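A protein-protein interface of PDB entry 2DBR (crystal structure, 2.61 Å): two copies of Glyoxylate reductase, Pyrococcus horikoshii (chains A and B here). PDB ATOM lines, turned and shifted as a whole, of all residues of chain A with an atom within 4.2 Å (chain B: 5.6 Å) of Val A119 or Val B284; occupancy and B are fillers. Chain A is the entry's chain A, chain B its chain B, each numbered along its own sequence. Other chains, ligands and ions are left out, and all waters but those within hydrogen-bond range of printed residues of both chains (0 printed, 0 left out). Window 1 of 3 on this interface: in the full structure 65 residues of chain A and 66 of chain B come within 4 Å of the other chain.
O of Ile B289 is in hydrogen-bond range of NH2 of Arg A117, at 3.1 Å.
N of Leu B285 is in hydrogen-bond range of OD2 of Asp A123.
The backbone carbonyl oxygen (O) of Ala A114 is in hydrogen-bond range of the backbone NH (N) of Val A119 (3.3 Å).
O of Ala B262 sits at hydrogen-bond distance from N of Val B284 (2.9 Å).
The backbone NH (N) of Leu B264 sits at hydrogen-bond distance from the backbone carbonyl oxygen (O) of Val B284.
N of Ile B289 lies within hydrogen-bond range of OD1 of Asp B265 (2.7 Å).
CD1 of Leu B107 touches CB of Arg A117, at 3.9 Å.
Ala B110 touches Val A119.
Val A119 touches Val B284 (CG1 to CG1, 3.8 Å).
Gly A122 touches Leu B285.
CG1 of Val B120 touches CG of Asp A123, at 3.5 Å.
Asp A123 touches Val B284 (OD2 to CA, 3.5 Å).
Of chain B, only Ala B110 (3.8 Å) and Val B284 (3.8 Å) come within 4 Å of Val A119.
Printed residues of chain B within 4 Å of Gly A122: Leu B285.
Printed residues of chain B within 4 Å of Asp A123: Val B120 (3.5 Å), Val B284 (3.5 Å) and Leu B285 (2.8 Å).
Of the printed residues of chain A, Ala B110 touches Val A119.
Printed residues of chain A within 4 Å of Val B120: Asp A123.
Val B284 touches two residues of chain A.
Of the printed residues of chain A, Ile B289 touches Arg A117.
The nearest printed residue of chain A that does not touch Val B284 is Val A120 (6.4 Å).
Of the 8 printed residues of chain A, 4 touch a printed residue of chain B.
Printed residues of chain B that touch a printed residue of chain A: Leu B107, Ala B110, Val B120, Val B284, Leu B285 and Ile B289.
Among the printed residues, 8 pairs touch across the chains.
Positions printed for both chains: 114 and 120.
Of the 8 pairs that touch across the chains among the printed residues, none has its exchanged pair printed and touching as well.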
ATOM      1  N   ALA A 114     -29.418  22.831 -35.210  1.00  0.00           N
ATOM      2  CA  ALA A 114     -28.830  23.594 -34.122  1.00  0.00           C
ATOM      3  C   ALA A 114     -29.250  25.062 -34.165  1.00  0.00           C
ATOM      4  O   ALA A 114     -29.560  25.654 -33.139  1.00  0.00           O
ATOM      5  CB  ALA A 114     -27.330  23.502 -34.185  1.00  0.00           C
ATOM      6  N   ARG A 117     -33.053  25.534 -33.404  1.00  0.00           N
ATOM      7  CA  ARG A 117     -33.474  25.149 -32.044  1.00  0.00           C
ATOM      8  C   ARG A 117     -32.678  25.699 -30.852  1.00  0.00           C
ATOM      9  O   ARG A 117     -32.984  25.381 -29.699  1.00  0.00           O
ATOM     10  CB  ARG A 117     -33.560  23.621 -31.940  1.00  0.00           C
ATOM     11  CG  ARG A 117     -34.527  23.016 -32.948  1.00  0.00           C
ATOM     12  CD  ARG A 117     -35.915  23.604 -32.775  1.00  0.00           C
ATOM     13  NE  ARG A 117     -36.413  23.307 -31.437  1.00  0.00           N
ATOM     14  CZ  ARG A 117     -36.980  22.157 -31.096  1.00  0.00           C
ATOM     15  NH1 ARG A 117     -37.138  21.203 -32.004  1.00  0.00           N
ATOM     16  NH2 ARG A 117     -37.349  21.945 -29.842  1.00  0.00           N
ATOM     17  N   HIS A 118     -31.662  26.514 -31.127  1.00  0.00           N
ATOM     18  CA  HIS A 118     -30.864  27.138 -30.073  1.00  0.00           C
ATOM     19  C   HIS A 118     -29.961  26.202 -29.292  1.00  0.00           C
ATOM     20  O   HIS A 118     -29.658  26.462 -28.125  1.00  0.00           O
ATOM     21  CB  HIS A 118     -31.780  27.859 -29.089  1.00  0.00           C
ATOM     22  CG  HIS A 118     -32.813  28.713 -29.753  1.00  0.00           C
ATOM     23  ND1 HIS A 118     -32.500  29.890 -30.397  1.00  0.00           N
ATOM     24  CD2 HIS A 118     -34.144  28.533 -29.916  1.00  0.00           C
ATOM     25  CE1 HIS A 118     -33.596  30.398 -30.932  1.00  0.00           C
ATOM     26  NE2 HIS A 118     -34.607  29.595 -30.653  1.00  0.00           N
ATOM     27  N   VAL A 119     -29.518  25.125 -29.930  1.00  0.00           N
ATOM     28  CA  VAL A 119     -28.637  24.181 -29.264  1.00  0.00           C
ATOM     29  C   VAL A 119     -27.433  24.906 -28.666  1.00  0.00           C
ATOM     30  O   VAL A 119     -27.224  24.876 -27.454  1.00  0.00           O
ATOM     31  CB  VAL A 119     -28.120  23.098 -30.234  1.00  0.00           C
ATOM     32  CG1 VAL A 119     -27.202  22.149 -29.499  1.00  0.00           C
ATOM     33  CG2 VAL A 119     -29.279  22.329 -30.838  1.00  0.00           C
ATOM     34  N   VAL A 120     -26.655  25.569 -29.514  1.00  0.00           N
ATOM     35  CA  VAL A 120     -25.453  26.273 -29.075  1.00  0.00           C
ATOM     36  C   VAL A 120     -25.709  27.280 -27.957  1.00  0.00           C
ATOM     37  O   VAL A 120     -24.881  27.433 -27.060  1.00  0.00           O
ATOM     38  CB  VAL A 120     -24.752  26.993 -30.267  1.00  0.00           C
ATOM     39  CG1 VAL A 120     -23.441  27.624 -29.806  1.00  0.00           C
ATOM     40  CG2 VAL A 120     -24.489  26.004 -31.397  1.00  0.00           C
ATOM     41  N   LYS A 121     -26.846  27.965 -27.998  1.00  0.00           N
ATOM     42  CA  LYS A 121     -27.150  28.935 -26.948  1.00  0.00           C
ATOM     43  C   LYS A 121     -27.557  28.208 -25.676  1.00  0.00           C
ATOM     44  O   LYS A 121     -27.032  28.487 -24.601  1.00  0.00           O
ATOM     45  CB  LYS A 121     -28.270  29.891 -27.383  1.00  0.00           C
ATOM     46  CG  LYS A 121     -28.731  30.824 -26.269  1.00  0.00           C
ATOM     47  CD  LYS A 121     -29.616  31.970 -26.760  1.00  0.00           C
ATOM     48  CE  LYS A 121     -30.884  31.493 -27.445  1.00  0.00           C
ATOM     49  NZ  LYS A 121     -30.611  30.941 -28.808  1.00  0.00           N
ATOM     50  N   GLY A 122     -28.485  27.265 -25.801  1.00  0.00           N
ATOM     51  CA  GLY A 122     -28.929  26.515 -24.640  1.00  0.00           C
ATOM     52  C   GLY A 122     -27.770  25.886 -23.887  1.00  0.00           C
ATOM     53  O   GLY A 122     -27.716  25.928 -22.657  1.00  0.00           O
ATOM     54  N   ASP A 123     -26.833  25.308 -24.633  1.00  0.00           N
ATOM     55  CA  ASP A 123     -25.664  24.664 -24.044  1.00  0.00           C
ATOM     56  C   ASP A 123     -24.907  25.625 -23.144  1.00  0.00           C
ATOM     57  O   ASP A 123     -24.437  25.242 -22.075  1.00  0.00           O
ATOM     58  CB  ASP A 123     -24.747  24.148 -25.153  1.00  0.00           C
ATOM     59  CG  ASP A 123     -23.540  23.407 -24.625  1.00  0.00           C
ATOM     60  OD1 ASP A 123     -22.612  24.057 -24.085  1.00  0.00           O
ATOM     61  OD2 ASP A 123     -23.517  22.164 -24.756  1.00  0.00           O
ATOM     62  N   LEU B 107     -35.070  17.826 -32.184  1.00  0.00           N
ATOM     63  CA  LEU B 107     -34.016  18.082 -31.217  1.00  0.00           C
ATOM     64  C   LEU B 107     -33.128  16.860 -30.975  1.00  0.00           C
ATOM     65  O   LEU B 107     -31.913  16.993 -30.766  1.00  0.00           O
ATOM     66  CB  LEU B 107     -34.633  18.550 -29.899  1.00  0.00           C
ATOM     67  CG  LEU B 107     -33.610  19.171 -28.954  1.00  0.00           C
ATOM     68  CD1 LEU B 107     -33.259  20.560 -29.462  1.00  0.00           C
ATOM     69  CD2 LEU B 107     -34.170  19.239 -27.548  1.00  0.00           C
ATOM     70  N   ALA B 110     -30.853  17.122 -33.546  1.00  0.00           N
ATOM     71  CA  ALA B 110     -30.002  18.297 -33.385  1.00  0.00           C
ATOM     72  C   ALA B 110     -28.840  17.900 -32.495  1.00  0.00           C
ATOM     73  O   ALA B 110     -27.682  18.251 -32.748  1.00  0.00           O
ATOM     74  CB  ALA B 110     -30.779  19.442 -32.742  1.00  0.00           C
ATOM     75  N   LEU B 111     -29.159  17.146 -31.448  1.00  0.00           N
ATOM     76  CA  LEU B 111     -28.151  16.695 -30.499  1.00  0.00           C
ATOM     77  C   LEU B 111     -27.221  15.651 -31.099  1.00  0.00           C
ATOM     78  O   LEU B 111     -25.998  15.740 -30.969  1.00  0.00           O
ATOM     79  CB  LEU B 111     -28.839  16.147 -29.255  1.00  0.00           C
ATOM     80  CG  LEU B 111     -29.518  17.248 -28.444  1.00  0.00           C
ATOM     81  CD1 LEU B 111     -30.368  16.637 -27.333  1.00  0.00           C
ATOM     82  CD2 LEU B 111     -28.445  18.181 -27.870  1.00  0.00           C
ATOM     83  N   ALA B 114     -24.981  17.588 -33.513  1.00  0.00           N
ATOM     84  CA  ALA B 114     -24.111  18.562 -32.861  1.00  0.00           C
ATOM     85  C   ALA B 114     -23.048  17.886 -32.012  1.00  0.00           C
ATOM     86  O   ALA B 114     -21.933  18.397 -31.889  1.00  0.00           O
ATOM     87  CB  ALA B 114     -24.932  19.507 -32.000  1.00  0.00           C
ATOM     88  N   THR B 115     -23.394  16.749 -31.409  1.00  0.00           N
ATOM     89  CA  THR B 115     -22.440  16.025 -30.577  1.00  0.00           C
ATOM     90  C   THR B 115     -21.445  15.299 -31.467  1.00  0.00           C
ATOM     91  O   THR B 115     -20.246  15.305 -31.209  1.00  0.00           O
ATOM     92  CB  THR B 115     -23.123  14.964 -29.685  1.00  0.00           C
ATOM     93  OG1 THR B 115     -24.140  15.577 -28.890  1.00  0.00           O
ATOM     94  CG2 THR B 115     -22.103  14.311 -28.773  1.00  0.00           C
ATOM     95  N   VAL B 120     -20.995  22.445 -30.889  1.00  0.00           N
ATOM     96  CA  VAL B 120     -20.925  23.355 -29.753  1.00  0.00           C
ATOM     97  C   VAL B 120     -19.495  23.826 -29.466  1.00  0.00           C
ATOM     98  O   VAL B 120     -19.264  24.998 -29.146  1.00  0.00           O
ATOM     99  CB  VAL B 120     -21.521  22.713 -28.474  1.00  0.00           C
ATOM    100  CG1 VAL B 120     -21.315  23.638 -27.278  1.00  0.00           C
ATOM    101  CG2 VAL B 120     -23.006  22.459 -28.668  1.00  0.00           C
ATOM    102  N   ALA B 262     -21.932  12.434 -25.525  1.00  0.00           N
ATOM    103  CA  ALA B 262     -23.347  12.406 -25.190  1.00  0.00           C
ATOM    104  C   ALA B 262     -24.006  13.761 -25.346  1.00  0.00           C
ATOM    105  O   ALA B 262     -23.428  14.789 -24.989  1.00  0.00           O
ATOM    106  CB  ALA B 262     -23.532  11.920 -23.749  1.00  0.00           C
ATOM    107  N   GLY B 263     -25.223  13.741 -25.875  1.00  0.00           N
ATOM    108  CA  GLY B 263     -26.004  14.954 -26.043  1.00  0.00           C
ATOM    109  C   GLY B 263     -27.179  14.795 -25.099  1.00  0.00           C
ATOM    110  O   GLY B 263     -28.051  13.954 -25.316  1.00  0.00           O
ATOM    111  N   LEU B 264     -27.216  15.598 -24.049  1.00  0.00           N
ATOM    112  CA  LEU B 264     -28.274  15.457 -23.069  1.00  0.00           C
ATOM    113  C   LEU B 264     -29.226  16.633 -22.991  1.00  0.00           C
ATOM    114  O   LEU B 264     -28.798  17.774 -22.825  1.00  0.00           O
ATOM    115  CB  LEU B 264     -27.643  15.225 -21.695  1.00  0.00           C
ATOM    116  CG  LEU B 264     -26.429  14.292 -21.751  1.00  0.00           C
ATOM    117  CD1 LEU B 264     -25.656  14.362 -20.437  1.00  0.00           C
ATOM    118  CD2 LEU B 264     -26.889  12.872 -22.079  1.00  0.00           C
ATOM    119  N   ASP B 265     -30.519  16.351 -23.107  1.00  0.00           N
ATOM    120  CA  ASP B 265     -31.525  17.399 -23.010  1.00  0.00           C
ATOM    121  C   ASP B 265     -32.182  17.340 -21.644  1.00  0.00           C
ATOM    122  O   ASP B 265     -32.751  18.322 -21.191  1.00  0.00           O
ATOM    123  CB  ASP B 265     -32.611  17.250 -24.076  1.00  0.00           C
ATOM    124  CG  ASP B 265     -33.698  18.316 -23.941  1.00  0.00           C
ATOM    125  OD1 ASP B 265     -33.342  19.503 -23.810  1.00  0.00           O
ATOM    126  OD2 ASP B 265     -34.897  17.975 -23.965  1.00  0.00           O
ATOM    127  N   ASN B 282     -16.992  16.581 -25.045  1.00  0.00           N
ATOM    128  CA  ASN B 282     -17.714  15.601 -25.846  1.00  0.00           C
ATOM    129  C   ASN B 282     -19.119  15.413 -25.288  1.00  0.00           C
ATOM    130  O   ASN B 282     -19.712  14.334 -25.368  1.00  0.00           O
ATOM    131  CB  ASN B 282     -16.945  14.278 -25.883  1.00  0.00           C
ATOM    132  CG  ASN B 282     -16.421  13.872 -24.525  1.00  0.00           C
ATOM    133  OD1 ASN B 282     -16.350  14.692 -23.605  1.00  0.00           O
ATOM    134  ND2 ASN B 282     -16.035  12.606 -24.390  1.00  0.00           N
ATOM    135  N   VAL B 283     -19.647  16.497 -24.731  1.00  0.00           N
ATOM    136  CA  VAL B 283     -20.985  16.505 -24.161  1.00  0.00           C
ATOM    137  C   VAL B 283     -21.694  17.784 -24.596  1.00  0.00           C
ATOM    138  O   VAL B 283     -21.165  18.879 -24.432  1.00  0.00           O
ATOM    139  CB  VAL B 283     -20.932  16.486 -22.625  1.00  0.00           C
ATOM    140  CG1 VAL B 283     -22.308  16.205 -22.066  1.00  0.00           C
ATOM    141  CG2 VAL B 283     -19.935  15.458 -22.158  1.00  0.00           C
ATOM    142  N   VAL B 284     -22.888  17.642 -25.153  1.00  0.00           N
ATOM    143  CA  VAL B 284     -23.676  18.781 -25.596  1.00  0.00           C
ATOM    144  C   VAL B 284     -24.883  18.802 -24.673  1.00  0.00           C
ATOM    145  O   VAL B 284     -25.522  17.774 -24.468  1.00  0.00           O
ATOM    146  CB  VAL B 284     -24.114  18.609 -27.079  1.00  0.00           C
ATOM    147  CG1 VAL B 284     -25.122  19.675 -27.470  1.00  0.00           C
ATOM    148  CG2 VAL B 284     -22.897  18.692 -27.983  1.00  0.00           C
ATOM    149  N   LEU B 285     -25.194  19.968 -24.116  1.00  0.00           N
ATOM    150  CA  LEU B 285     -26.297  20.088 -23.173  1.00  0.00           C
ATOM    151  C   LEU B 285     -27.328  21.125 -23.572  1.00  0.00           C
ATOM    152  O   LEU B 285     -26.978  22.163 -24.118  1.00  0.00           O
ATOM    153  CB  LEU B 285     -25.746  20.475 -21.803  1.00  0.00           C
ATOM    154  CG  LEU B 285     -24.325  20.010 -21.474  1.00  0.00           C
ATOM    155  CD1 LEU B 285     -23.798  20.857 -20.329  1.00  0.00           C
ATOM    156  CD2 LEU B 285     -24.305  18.516 -21.141  1.00  0.00           C
ATOM    157  N   THR B 286     -28.595  20.838 -23.282  1.00  0.00           N
ATOM    158  CA  THR B 286     -29.700  21.754 -23.553  1.00  0.00           C
ATOM    159  C   THR B 286     -30.645  21.697 -22.341  1.00  0.00           C
ATOM    160  O   THR B 286     -30.889  20.620 -21.793  1.00  0.00           O
ATOM    161  CB  THR B 286     -30.448  21.384 -24.863  1.00  0.00           C
ATOM    162  OG1 THR B 286     -30.843  20.006 -24.850  1.00  0.00           O
ATOM    163  CG2 THR B 286     -29.544  21.618 -26.046  1.00  0.00           C
ATOM    164  N   ILE B 289     -35.311  21.302 -23.574  1.00  0.00           N
ATOM    165  CA  ILE B 289     -36.049  22.062 -24.570  1.00  0.00           C
ATOM    166  C   ILE B 289     -36.587  21.177 -25.683  1.00  0.00           C
ATOM    167  O   ILE B 289     -36.881  21.658 -26.781  1.00  0.00           O
ATOM    168  CB  ILE B 289     -35.145  23.131 -25.185  1.00  0.00           C
ATOM    169  CG1 ILE B 289     -34.091  22.468 -26.083  1.00  0.00           C
ATOM    170  CG2 ILE B 289     -34.456  23.920 -24.072  1.00  0.00           C
ATOM    171  CD1 ILE B 289     -32.930  23.377 -26.462  1.00  0.00           C
